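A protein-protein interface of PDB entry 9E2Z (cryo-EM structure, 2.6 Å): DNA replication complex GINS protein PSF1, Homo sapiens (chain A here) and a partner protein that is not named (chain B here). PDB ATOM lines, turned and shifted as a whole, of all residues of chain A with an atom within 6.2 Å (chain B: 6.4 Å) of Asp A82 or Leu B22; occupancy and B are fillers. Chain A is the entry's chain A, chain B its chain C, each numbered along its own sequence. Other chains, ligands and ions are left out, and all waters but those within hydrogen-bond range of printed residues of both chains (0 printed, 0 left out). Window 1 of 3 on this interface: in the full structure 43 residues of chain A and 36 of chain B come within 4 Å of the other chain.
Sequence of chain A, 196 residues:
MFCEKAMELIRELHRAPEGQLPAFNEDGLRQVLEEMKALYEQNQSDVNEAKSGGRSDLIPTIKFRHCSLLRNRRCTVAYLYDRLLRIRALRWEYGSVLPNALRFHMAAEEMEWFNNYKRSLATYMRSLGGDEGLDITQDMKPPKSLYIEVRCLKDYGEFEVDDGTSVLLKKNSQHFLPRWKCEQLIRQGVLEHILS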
ATOM      1  N   ILE A  10      10.740  -0.121 -10.654  1.00  0.00           N
ATOM      2  CA  ILE A  10      12.006   0.062 -11.358  1.00  0.00           C
ATOM      3  C   ILE A  10      12.887  -1.175 -11.221  1.00  0.00           C
ATOM      4  O   ILE A  10      13.507  -1.624 -12.194  1.00  0.00           O
ATOM      5  CB  ILE A  10      12.719   1.324 -10.839  1.00  0.00           C
ATOM      6  CG1 ILE A  10      11.903   2.574 -11.178  1.00  0.00           C
ATOM      7  CG2 ILE A  10      14.122   1.418 -11.410  1.00  0.00           C
ATOM      8  CD1 ILE A  10      11.626   2.765 -12.650  1.00  0.00           C
ATOM      9  N   LEU A  13      12.273  -4.163 -13.652  1.00  0.00           N
ATOM     10  CA  LEU A  13      12.845  -4.015 -14.985  1.00  0.00           C
ATOM     11  C   LEU A  13      14.363  -4.081 -14.948  1.00  0.00           C
ATOM     12  O   LEU A  13      14.984  -4.679 -15.835  1.00  0.00           O
ATOM     13  CB  LEU A  13      12.393  -2.697 -15.609  1.00  0.00           C
ATOM     14  CG  LEU A  13      10.983  -2.628 -16.187  1.00  0.00           C
ATOM     15  CD1 LEU A  13      10.823  -1.334 -16.946  1.00  0.00           C
ATOM     16  CD2 LEU A  13      10.684  -3.812 -17.081  1.00  0.00           C
ATOM     17  N   HIS A  14      14.986  -3.465 -13.943  1.00  0.00           N
ATOM     18  CA  HIS A  14      16.443  -3.467 -13.885  1.00  0.00           C
ATOM     19  C   HIS A  14      16.991  -4.886 -13.799  1.00  0.00           C
ATOM     20  O   HIS A  14      18.073  -5.174 -14.319  1.00  0.00           O
ATOM     21  CB  HIS A  14      16.926  -2.638 -12.699  1.00  0.00           C
ATOM     22  CG  HIS A  14      18.416  -2.563 -12.585  1.00  0.00           C
ATOM     23  ND1 HIS A  14      19.187  -1.779 -13.415  1.00  0.00           N
ATOM     24  CD2 HIS A  14      19.278  -3.173 -11.738  1.00  0.00           C
ATOM     25  CE1 HIS A  14      20.459  -1.908 -13.085  1.00  0.00           C
ATOM     26  NE2 HIS A  14      20.541  -2.750 -12.070  1.00  0.00           N
ATOM     27  N   LEU A  21      10.245  -8.801 -21.850  1.00  0.00           N
ATOM     28  CA  LEU A  21       9.108  -8.055 -21.340  1.00  0.00           C
ATOM     29  C   LEU A  21       8.442  -8.846 -20.225  1.00  0.00           C
ATOM     30  O   LEU A  21       7.878  -9.914 -20.497  1.00  0.00           O
ATOM     31  CB  LEU A  21       8.115  -7.779 -22.465  1.00  0.00           C
ATOM     32  CG  LEU A  21       7.062  -6.703 -22.213  1.00  0.00           C
ATOM     33  CD1 LEU A  21       7.696  -5.333 -22.095  1.00  0.00           C
ATOM     34  CD2 LEU A  21       6.034  -6.727 -23.328  1.00  0.00           C
ATOM     35  N   VAL A  77       6.944   7.047 -15.065  1.00  0.00           N
ATOM     36  CA  VAL A  77       7.187   7.337 -16.473  1.00  0.00           C
ATOM     37  C   VAL A  77       8.379   6.541 -16.984  1.00  0.00           C
ATOM     38  O   VAL A  77       8.355   6.023 -18.105  1.00  0.00           O
ATOM     39  CB  VAL A  77       7.381   8.848 -16.684  1.00  0.00           C
ATOM     40  CG1 VAL A  77       7.845   9.128 -18.101  1.00  0.00           C
ATOM     41  CG2 VAL A  77       6.095   9.583 -16.395  1.00  0.00           C
ATOM     42  N   ALA A  78       9.440   6.435 -16.183  1.00  0.00           N
ATOM     43  CA  ALA A  78      10.598   5.660 -16.612  1.00  0.00           C
ATOM     44  C   ALA A  78      10.228   4.201 -16.840  1.00  0.00           C
ATOM     45  O   ALA A  78      10.636   3.598 -17.840  1.00  0.00           O
ATOM     46  CB  ALA A  78      11.716   5.775 -15.579  1.00  0.00           C
ATOM     47  N   TYR A  79       9.451   3.620 -15.926  1.00  0.00           N
ATOM     48  CA  TYR A  79       9.011   2.237 -16.084  1.00  0.00           C
ATOM     49  C   TYR A  79       8.252   2.049 -17.393  1.00  0.00           C
ATOM     50  O   TYR A  79       8.569   1.159 -18.200  1.00  0.00           O
ATOM     51  CB  TYR A  79       8.145   1.857 -14.880  1.00  0.00           C
ATOM     52  CG  TYR A  79       7.429   0.537 -14.991  1.00  0.00           C
ATOM     53  CD1 TYR A  79       8.080  -0.651 -14.721  1.00  0.00           C
ATOM     54  CD2 TYR A  79       6.094   0.482 -15.355  1.00  0.00           C
ATOM     55  CE1 TYR A  79       7.427  -1.853 -14.819  1.00  0.00           C
ATOM     56  CE2 TYR A  79       5.439  -0.712 -15.456  1.00  0.00           C
ATOM     57  CZ  TYR A  79       6.106  -1.878 -15.184  1.00  0.00           C
ATOM     58  OH  TYR A  79       5.453  -3.080 -15.284  1.00  0.00           O
ATOM     59  N   LEU A  80       7.260   2.908 -17.632  1.00  0.00           N
ATOM     60  CA  LEU A  80       6.448   2.776 -18.838  1.00  0.00           C
ATOM     61  C   LEU A  80       7.293   2.941 -20.099  1.00  0.00           C
ATOM     62  O   LEU A  80       7.134   2.189 -21.069  1.00  0.00           O
ATOM     63  CB  LEU A  80       5.312   3.797 -18.805  1.00  0.00           C
ATOM     64  CG  LEU A  80       4.294   3.612 -17.679  1.00  0.00           C
ATOM     65  CD1 LEU A  80       3.308   4.757 -17.654  1.00  0.00           C
ATOM     66  CD2 LEU A  80       3.564   2.296 -17.819  1.00  0.00           C
ATOM     67  N   TYR A  81       8.209   3.910 -20.098  1.00  0.00           N
ATOM     68  CA  TYR A  81       9.020   4.165 -21.283  1.00  0.00           C
ATOM     69  C   TYR A  81       9.963   3.005 -21.583  1.00  0.00           C
ATOM     70  O   TYR A  81      10.155   2.637 -22.748  1.00  0.00           O
ATOM     71  CB  TYR A  81       9.801   5.460 -21.096  1.00  0.00           C
ATOM     72  CG  TYR A  81      10.467   5.960 -22.349  1.00  0.00           C
ATOM     73  CD1 TYR A  81       9.730   6.559 -23.357  1.00  0.00           C
ATOM     74  CD2 TYR A  81      11.833   5.835 -22.524  1.00  0.00           C
ATOM     75  CE1 TYR A  81      10.337   7.016 -24.501  1.00  0.00           C
ATOM     76  CE2 TYR A  81      12.447   6.288 -23.661  1.00  0.00           C
ATOM     77  CZ  TYR A  81      11.697   6.880 -24.647  1.00  0.00           C
ATOM     78  OH  TYR A  81      12.313   7.334 -25.785  1.00  0.00           O
ATOM     79  N   ASP A  82      10.575   2.422 -20.551  1.00  0.00           N
ATOM     80  CA  ASP A  82      11.444   1.273 -20.779  1.00  0.00           C
ATOM     81  C   ASP A  82      10.655   0.102 -21.348  1.00  0.00           C
ATOM     82  O   ASP A  82      11.132  -0.611 -22.246  1.00  0.00           O
ATOM     83  CB  ASP A  82      12.140   0.887 -19.476  1.00  0.00           C
ATOM     84  CG  ASP A  82      13.171  -0.202 -19.665  1.00  0.00           C
ATOM     85  OD1 ASP A  82      12.789  -1.385 -19.713  1.00  0.00           O
ATOM     86  OD2 ASP A  82      14.366   0.125 -19.771  1.00  0.00           O
ATOM     87  N   ARG A  83       9.437  -0.108 -20.846  1.00  0.00           N
ATOM     88  CA  ARG A  83       8.592  -1.137 -21.440  1.00  0.00           C
ATOM     89  C   ARG A  83       8.337  -0.847 -22.914  1.00  0.00           C
ATOM     90  O   ARG A  83       8.360  -1.761 -23.747  1.00  0.00           O
ATOM     91  CB  ARG A  83       7.275  -1.241 -20.676  1.00  0.00           C
ATOM     92  CG  ARG A  83       7.406  -1.892 -19.317  1.00  0.00           C
ATOM     93  CD  ARG A  83       6.049  -2.169 -18.699  1.00  0.00           C
ATOM     94  NE  ARG A  83       5.249  -3.082 -19.506  1.00  0.00           N
ATOM     95  CZ  ARG A  83       5.254  -4.401 -19.381  1.00  0.00           C
ATOM     96  NH1 ARG A  83       6.015  -5.010 -18.490  1.00  0.00           N
ATOM     97  NH2 ARG A  83       4.479  -5.129 -20.177  1.00  0.00           N
ATOM     98  N   LEU A  84       8.086   0.417 -23.253  1.00  0.00           N
ATOM     99  CA  LEU A  84       7.868   0.766 -24.656  1.00  0.00           C
ATOM    100  C   LEU A  84       9.094   0.451 -25.502  1.00  0.00           C
ATOM    101  O   LEU A  84       8.966  -0.003 -26.641  1.00  0.00           O
ATOM    102  CB  LEU A  84       7.508   2.244 -24.793  1.00  0.00           C
ATOM    103  CG  LEU A  84       6.073   2.684 -24.512  1.00  0.00           C
ATOM    104  CD1 LEU A  84       5.883   4.105 -24.993  1.00  0.00           C
ATOM    105  CD2 LEU A  84       5.053   1.763 -25.156  1.00  0.00           C
ATOM    106  N   LEU A  85      10.289   0.710 -24.974  1.00  0.00           N
ATOM    107  CA  LEU A  85      11.503   0.393 -25.724  1.00  0.00           C
ATOM    108  C   LEU A  85      11.607  -1.101 -26.004  1.00  0.00           C
ATOM    109  O   LEU A  85      11.948  -1.515 -27.121  1.00  0.00           O
ATOM    110  CB  LEU A  85      12.738   0.873 -24.966  1.00  0.00           C
ATOM    111  CG  LEU A  85      12.872   2.378 -24.746  1.00  0.00           C
ATOM    112  CD1 LEU A  85      14.017   2.661 -23.803  1.00  0.00           C
ATOM    113  CD2 LEU A  85      13.074   3.095 -26.056  1.00  0.00           C
ATOM    114  N   ARG A  86      11.310  -1.929 -25.003  1.00  0.00           N
ATOM    115  CA  ARG A  86      11.354  -3.373 -25.226  1.00  0.00           C
ATOM    116  C   ARG A  86      10.325  -3.805 -26.272  1.00  0.00           C
ATOM    117  O   ARG A  86      10.618  -4.617 -27.166  1.00  0.00           O
ATOM    118  CB  ARG A  86      11.136  -4.100 -23.903  1.00  0.00           C
ATOM    119  CG  ARG A  86      12.218  -3.813 -22.888  1.00  0.00           C
ATOM    120  CD  ARG A  86      11.988  -4.545 -21.591  1.00  0.00           C
ATOM    121  NE  ARG A  86      12.762  -3.947 -20.511  1.00  0.00           N
ATOM    122  CZ  ARG A  86      13.628  -4.589 -19.740  1.00  0.00           C
ATOM    123  NH1 ARG A  86      13.833  -5.889 -19.856  1.00  0.00           N
ATOM    124  NH2 ARG A  86      14.305  -3.907 -18.822  1.00  0.00           N
ATOM    125  N   ILE A  87       9.116  -3.251 -26.192  1.00  0.00           N
ATOM    126  CA  ILE A  87       8.087  -3.581 -27.172  1.00  0.00           C
ATOM    127  C   ILE A  87       8.538  -3.175 -28.570  1.00  0.00           C
ATOM    128  O   ILE A  87       8.336  -3.909 -29.541  1.00  0.00           O
ATOM    129  CB  ILE A  87       6.756  -2.916 -26.787  1.00  0.00           C
ATOM    130  CG1 ILE A  87       6.179  -3.587 -25.541  1.00  0.00           C
ATOM    131  CG2 ILE A  87       5.769  -2.998 -27.926  1.00  0.00           C
ATOM    132  CD1 ILE A  87       5.309  -2.683 -24.722  1.00  0.00           C
ATOM    133  N   TYR B   5      17.337  -3.405 -28.649  1.00  0.00           N
ATOM    134  CA  TYR B   5      16.881  -2.818 -27.397  1.00  0.00           C
ATOM    135  C   TYR B   5      18.048  -2.092 -26.747  1.00  0.00           C
ATOM    136  O   TYR B   5      19.073  -2.708 -26.439  1.00  0.00           O
ATOM    137  CB  TYR B   5      16.334  -3.871 -26.438  1.00  0.00           C
ATOM    138  CG  TYR B   5      16.197  -3.348 -25.024  1.00  0.00           C
ATOM    139  CD1 TYR B   5      15.379  -2.265 -24.744  1.00  0.00           C
ATOM    140  CD2 TYR B   5      16.897  -3.923 -23.976  1.00  0.00           C
ATOM    141  CE1 TYR B   5      15.253  -1.777 -23.464  1.00  0.00           C
ATOM    142  CE2 TYR B   5      16.781  -3.440 -22.693  1.00  0.00           C
ATOM    143  CZ  TYR B   5      15.956  -2.367 -22.442  1.00  0.00           C
ATOM    144  OH  TYR B   5      15.834  -1.879 -21.164  1.00  0.00           O
ATOM    145  N   ARG B   7      18.484   0.515 -23.578  1.00  0.00           N
ATOM    146  CA  ARG B   7      17.956   1.281 -22.464  1.00  0.00           C
ATOM    147  C   ARG B   7      18.494   2.707 -22.499  1.00  0.00           C
ATOM    148  O   ARG B   7      19.526   2.997 -23.104  1.00  0.00           O
ATOM    149  CB  ARG B   7      18.328   0.611 -21.143  1.00  0.00           C
ATOM    150  CG  ARG B   7      19.789   0.789 -20.767  1.00  0.00           C
ATOM    151  CD  ARG B   7      20.320  -0.362 -19.933  1.00  0.00           C
ATOM    152  NE  ARG B   7      20.311  -0.054 -18.507  1.00  0.00           N
ATOM    153  CZ  ARG B   7      19.664  -0.749 -17.578  1.00  0.00           C
ATOM    154  NH1 ARG B   7      18.937  -1.813 -17.883  1.00  0.00           N
ATOM    155  NH2 ARG B   7      19.749  -0.367 -16.308  1.00  0.00           N
ATOM    156  N   VAL B   8      17.774   3.609 -21.838  1.00  0.00           N
ATOM    157  CA  VAL B   8      18.248   4.981 -21.704  1.00  0.00           C
ATOM    158  C   VAL B   8      19.532   4.967 -20.886  1.00  0.00           C
ATOM    159  O   VAL B   8      19.615   4.313 -19.841  1.00  0.00           O
ATOM    160  CB  VAL B   8      17.182   5.872 -21.058  1.00  0.00           C
ATOM    161  CG1 VAL B   8      17.742   7.249 -20.789  1.00  0.00           C
ATOM    162  CG2 VAL B   8      15.960   5.951 -21.940  1.00  0.00           C
ATOM    163  N   ASN B  18      19.967  11.661 -16.021  1.00  0.00           N
ATOM    164  CA  ASN B  18      18.946  11.475 -17.044  1.00  0.00           C
ATOM    165  C   ASN B  18      17.619  11.070 -16.418  1.00  0.00           C
ATOM    166  O   ASN B  18      17.562  10.155 -15.593  1.00  0.00           O
ATOM    167  CB  ASN B  18      19.395  10.423 -18.057  1.00  0.00           C
ATOM    168  CG  ASN B  18      20.294  10.995 -19.132  1.00  0.00           C
ATOM    169  OD1 ASN B  18      20.329  12.203 -19.347  1.00  0.00           O
ATOM    170  ND2 ASN B  18      21.028  10.129 -19.813  1.00  0.00           N
ATOM    171  N   PHE B  19      16.549  11.742 -16.841  1.00  0.00           N
ATOM    172  CA  PHE B  19      15.241  11.555 -16.225  1.00  0.00           C
ATOM    173  C   PHE B  19      14.753  10.118 -16.361  1.00  0.00           C
ATOM    174  O   PHE B  19      14.181   9.560 -15.420  1.00  0.00           O
ATOM    175  CB  PHE B  19      14.249  12.526 -16.860  1.00  0.00           C
ATOM    176  CG  PHE B  19      12.907  12.565 -16.191  1.00  0.00           C
ATOM    177  CD1 PHE B  19      12.716  13.292 -15.031  1.00  0.00           C
ATOM    178  CD2 PHE B  19      11.827  11.898 -16.740  1.00  0.00           C
ATOM    179  CE1 PHE B  19      11.484  13.338 -14.427  1.00  0.00           C
ATOM    180  CE2 PHE B  19      10.593  11.942 -16.136  1.00  0.00           C
ATOM    181  CZ  PHE B  19      10.420  12.664 -14.982  1.00  0.00           C
ATOM    182  N   LEU B  20      14.971   9.500 -17.520  1.00  0.00           N
ATOM    183  CA  LEU B  20      14.416   8.191 -17.828  1.00  0.00           C
ATOM    184  C   LEU B  20      15.425   7.063 -17.651  1.00  0.00           C
ATOM    185  O   LEU B  20      15.203   5.963 -18.160  1.00  0.00           O
ATOM    186  CB  LEU B  20      13.868   8.182 -19.254  1.00  0.00           C
ATOM    187  CG  LEU B  20      12.703   9.131 -19.526  1.00  0.00           C
ATOM    188  CD1 LEU B  20      12.537   9.356 -21.017  1.00  0.00           C
ATOM    189  CD2 LEU B  20      11.429   8.591 -18.933  1.00  0.00           C
ATOM    190  N   SER B  21      16.517   7.304 -16.937  1.00  0.00           N
ATOM    191  CA  SER B  21      17.564   6.308 -16.759  1.00  0.00           C
ATOM    192  C   SER B  21      17.289   5.486 -15.503  1.00  0.00           C
ATOM    193  O   SER B  21      17.235   6.033 -14.398  1.00  0.00           O
ATOM    194  CB  SER B  21      18.930   6.981 -16.666  1.00  0.00           C
ATOM    195  OG  SER B  21      19.926   6.050 -16.293  1.00  0.00           O
ATOM    196  N   LEU B  22      17.127   4.174 -15.678  1.00  0.00           N
ATOM    197  CA  LEU B  22      16.906   3.293 -14.536  1.00  0.00           C
ATOM    198  C   LEU B  22      18.103   3.304 -13.595  1.00  0.00           C
ATOM    199  O   LEU B  22      17.943   3.311 -12.366  1.00  0.00           O
ATOM    200  CB  LEU B  22      16.628   1.871 -15.021  1.00  0.00           C
ATOM    201  CG  LEU B  22      15.491   1.685 -16.027  1.00  0.00           C
ATOM    202  CD1 LEU B  22      15.285   0.210 -16.313  1.00  0.00           C
ATOM    203  CD2 LEU B  22      14.209   2.314 -15.533  1.00  0.00           C
ATOM    204  N   ASP B  23      19.314   3.299 -14.157  1.00  0.00           N
ATOM    205  CA  ASP B  23      20.515   3.335 -13.332  1.00  0.00           C
ATOM    206  C   ASP B  23      20.547   4.584 -12.467  1.00  0.00           C
ATOM    207  O   ASP B  23      20.907   4.519 -11.290  1.00  0.00           O
ATOM    208  CB  ASP B  23      21.761   3.272 -14.212  1.00  0.00           C
ATOM    209  CG  ASP B  23      21.795   2.045 -15.094  1.00  0.00           C
ATOM    210  OD1 ASP B  23      22.192   0.970 -14.601  1.00  0.00           O
ATOM    211  OD2 ASP B  23      21.428   2.155 -16.283  1.00  0.00           O
ATOM    212  N   ASP B  24      20.182   5.733 -13.033  1.00  0.00           N
ATOM    213  CA  ASP B  24      20.206   6.970 -12.263  1.00  0.00           C
ATOM    214  C   ASP B  24      19.169   6.952 -11.146  1.00  0.00           C
ATOM    215  O   ASP B  24      19.422   7.462 -10.052  1.00  0.00           O
ATOM    216  CB  ASP B  24      19.986   8.164 -13.189  1.00  0.00           C
ATOM    217  CG  ASP B  24      21.229   8.529 -13.974  1.00  0.00           C
ATOM    218  OD1 ASP B  24      22.296   7.941 -13.717  1.00  0.00           O
ATOM    219  OD2 ASP B  24      21.138   9.400 -14.859  1.00  0.00           O
ATOM    220  N   ILE B  25      17.996   6.373 -11.401  1.00  0.00           N
ATOM    221  CA  ILE B  25      16.976   6.279 -10.360  1.00  0.00           C
ATOM    222  C   ILE B  25      17.465   5.397  -9.215  1.00  0.00           C
ATOM    223  O   ILE B  25      17.357   5.761  -8.034  1.00  0.00           O
ATOM    224  CB  ILE B  25      15.656   5.770 -10.968  1.00  0.00           C
ATOM    225  CG1 ILE B  25      14.991   6.890 -11.769  1.00  0.00           C
ATOM    226  CG2 ILE B  25      14.713   5.274  -9.898  1.00  0.00           C
ATOM    227  CD1 ILE B  25      13.970   6.414 -12.754  1.00  0.00           C
ATOM    228  N   LEU B  26      18.047   4.243  -9.545  1.00  0.00           N
ATOM    229  CA  LEU B  26      18.601   3.384  -8.505  1.00  0.00           C
ATOM    230  C   LEU B  26      19.723   4.085  -7.748  1.00  0.00           C
ATOM    231  O   LEU B  26      19.824   3.964  -6.523  1.00  0.00           O
ATOM    232  CB  LEU B  26      19.105   2.079  -9.113  1.00  0.00           C
ATOM    233  CG  LEU B  26      18.034   1.082  -9.555  1.00  0.00           C
ATOM    234  CD1 LEU B  26      18.623   0.073 -10.513  1.00  0.00           C
ATOM    235  CD2 LEU B  26      17.426   0.382  -8.362  1.00  0.00           C
ATOM    236  N   MET B  27      20.584   4.815  -8.461  1.00  0.00           N
ATOM    237  CA  MET B  27      21.689   5.505  -7.808  1.00  0.00           C
ATOM    238  C   MET B  27      21.180   6.564  -6.840  1.00  0.00           C
ATOM    239  O   MET B  27      21.670   6.669  -5.710  1.00  0.00           O
ATOM    240  CB  MET B  27      22.598   6.138  -8.862  1.00  0.00           C
ATOM    241  CG  MET B  27      23.678   7.059  -8.309  1.00  0.00           C
ATOM    242  SD  MET B  27      23.162   8.773  -8.095  1.00  0.00           S
ATOM    243  CE  MET B  27      22.740   9.229  -9.771  1.00  0.00           C
ATOM    244  N   HIS B 115      27.259   2.474  -7.582  1.00  0.00           N
ATOM    245  CA  HIS B 115      27.439   3.641  -8.441  1.00  0.00           C
ATOM    246  C   HIS B 115      28.392   4.629  -7.771  1.00  0.00           C
ATOM    247  O   HIS B 115      28.024   5.736  -7.388  1.00  0.00           O
ATOM    248  CB  HIS B 115      26.089   4.281  -8.743  1.00  0.00           C
ATOM    249  CG  HIS B 115      25.057   3.310  -9.220  1.00  0.00           C
ATOM    250  ND1 HIS B 115      24.895   2.989 -10.550  1.00  0.00           N
ATOM    251  CD2 HIS B 115      24.134   2.586  -8.544  1.00  0.00           C
ATOM    252  CE1 HIS B 115      23.916   2.111 -10.673  1.00  0.00           C
ATOM    253  NE2 HIS B 115      23.438   1.850  -9.471  1.00  0.00           N
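The guanidinium group (NH2) of Arg B7 is in hydrogen-bond range of a ring nitrogen (ND1) of His A14.
The side-chain hydroxyl (OH) of Tyr B5 is in hydrogen-bond range of the side-chain carboxylate (OD2) of Asp A82, 2.8 Å away.
The guanidinium group (NH2) of Arg A86 is in hydrogen-bond range of the side-chain hydroxyl (OH) of Tyr B5, at 3.5 Å.
The guanidinium group (NH2) of Arg A86 is in hydrogen-bond range of the backbone carbonyl oxygen (O) of Leu A13, 3.2 Å away.
The guanidinium group of Arg A86 is in salt-bridge range of the side-chain carboxylate of Asp A82, at 2.7 Å.
OD2 of Asp B23 lies within salt-bridge range of NH2 of Arg B7.
Among the printed residues, merely in contact across the chains: Ile A10 with Leu B22, His A14 with Asp B23, His A14 with Leu B26, Val A77 with Leu B20, Ala A78 with Leu B20, Ala A78 with Ile B25, Tyr A81 with Val B8, Tyr A81 with Leu B20, Asp A82 with Leu B22 and Leu A85 with Tyr B5.
Asp A82 touches just these residues of chain B: Tyr B5 (2.8 Å) and Leu B22 (3.6 Å).
Leu B22 touches two residues of chain A.
Of the printed residues of chain A, Val B8 touches Tyr A81 (3.9 Å).
Printed residues of chain A within 4 Å of Leu B26: His A14.
Printed residues of chain B within 4 Å of Val A77: Leu B20.
Asn B18 touches none of the printed residues of chain A.
Arg A83 touches none of the printed residues of chain B.
The nearest residue of chain B that does not touch Asp A82 is Arg B7 (4.2 Å).
Printed residues of chain A that touch a printed residue of chain B: Ile A10, His A14, Val A77, Ala A78, Tyr A81, Asp A82, Leu A85 and Arg A86.
Hydrophobic or aromatic side chains of chain A that line the printed part of chain B: Ile A10, His A14, Val A77, Ala A78, Tyr A81 and Leu A85.
Along chain A the printed residues that touch a printed residue of chain B span positions 10 to 86.
Hydrophobic or aromatic side chains of chain B within 4 Å of the printed part of chain A: Tyr B5, Val B8, Leu B20, Leu B22, Ile B25 and Leu B26.
Among the printed residues, 13 pairs touch across the chains.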
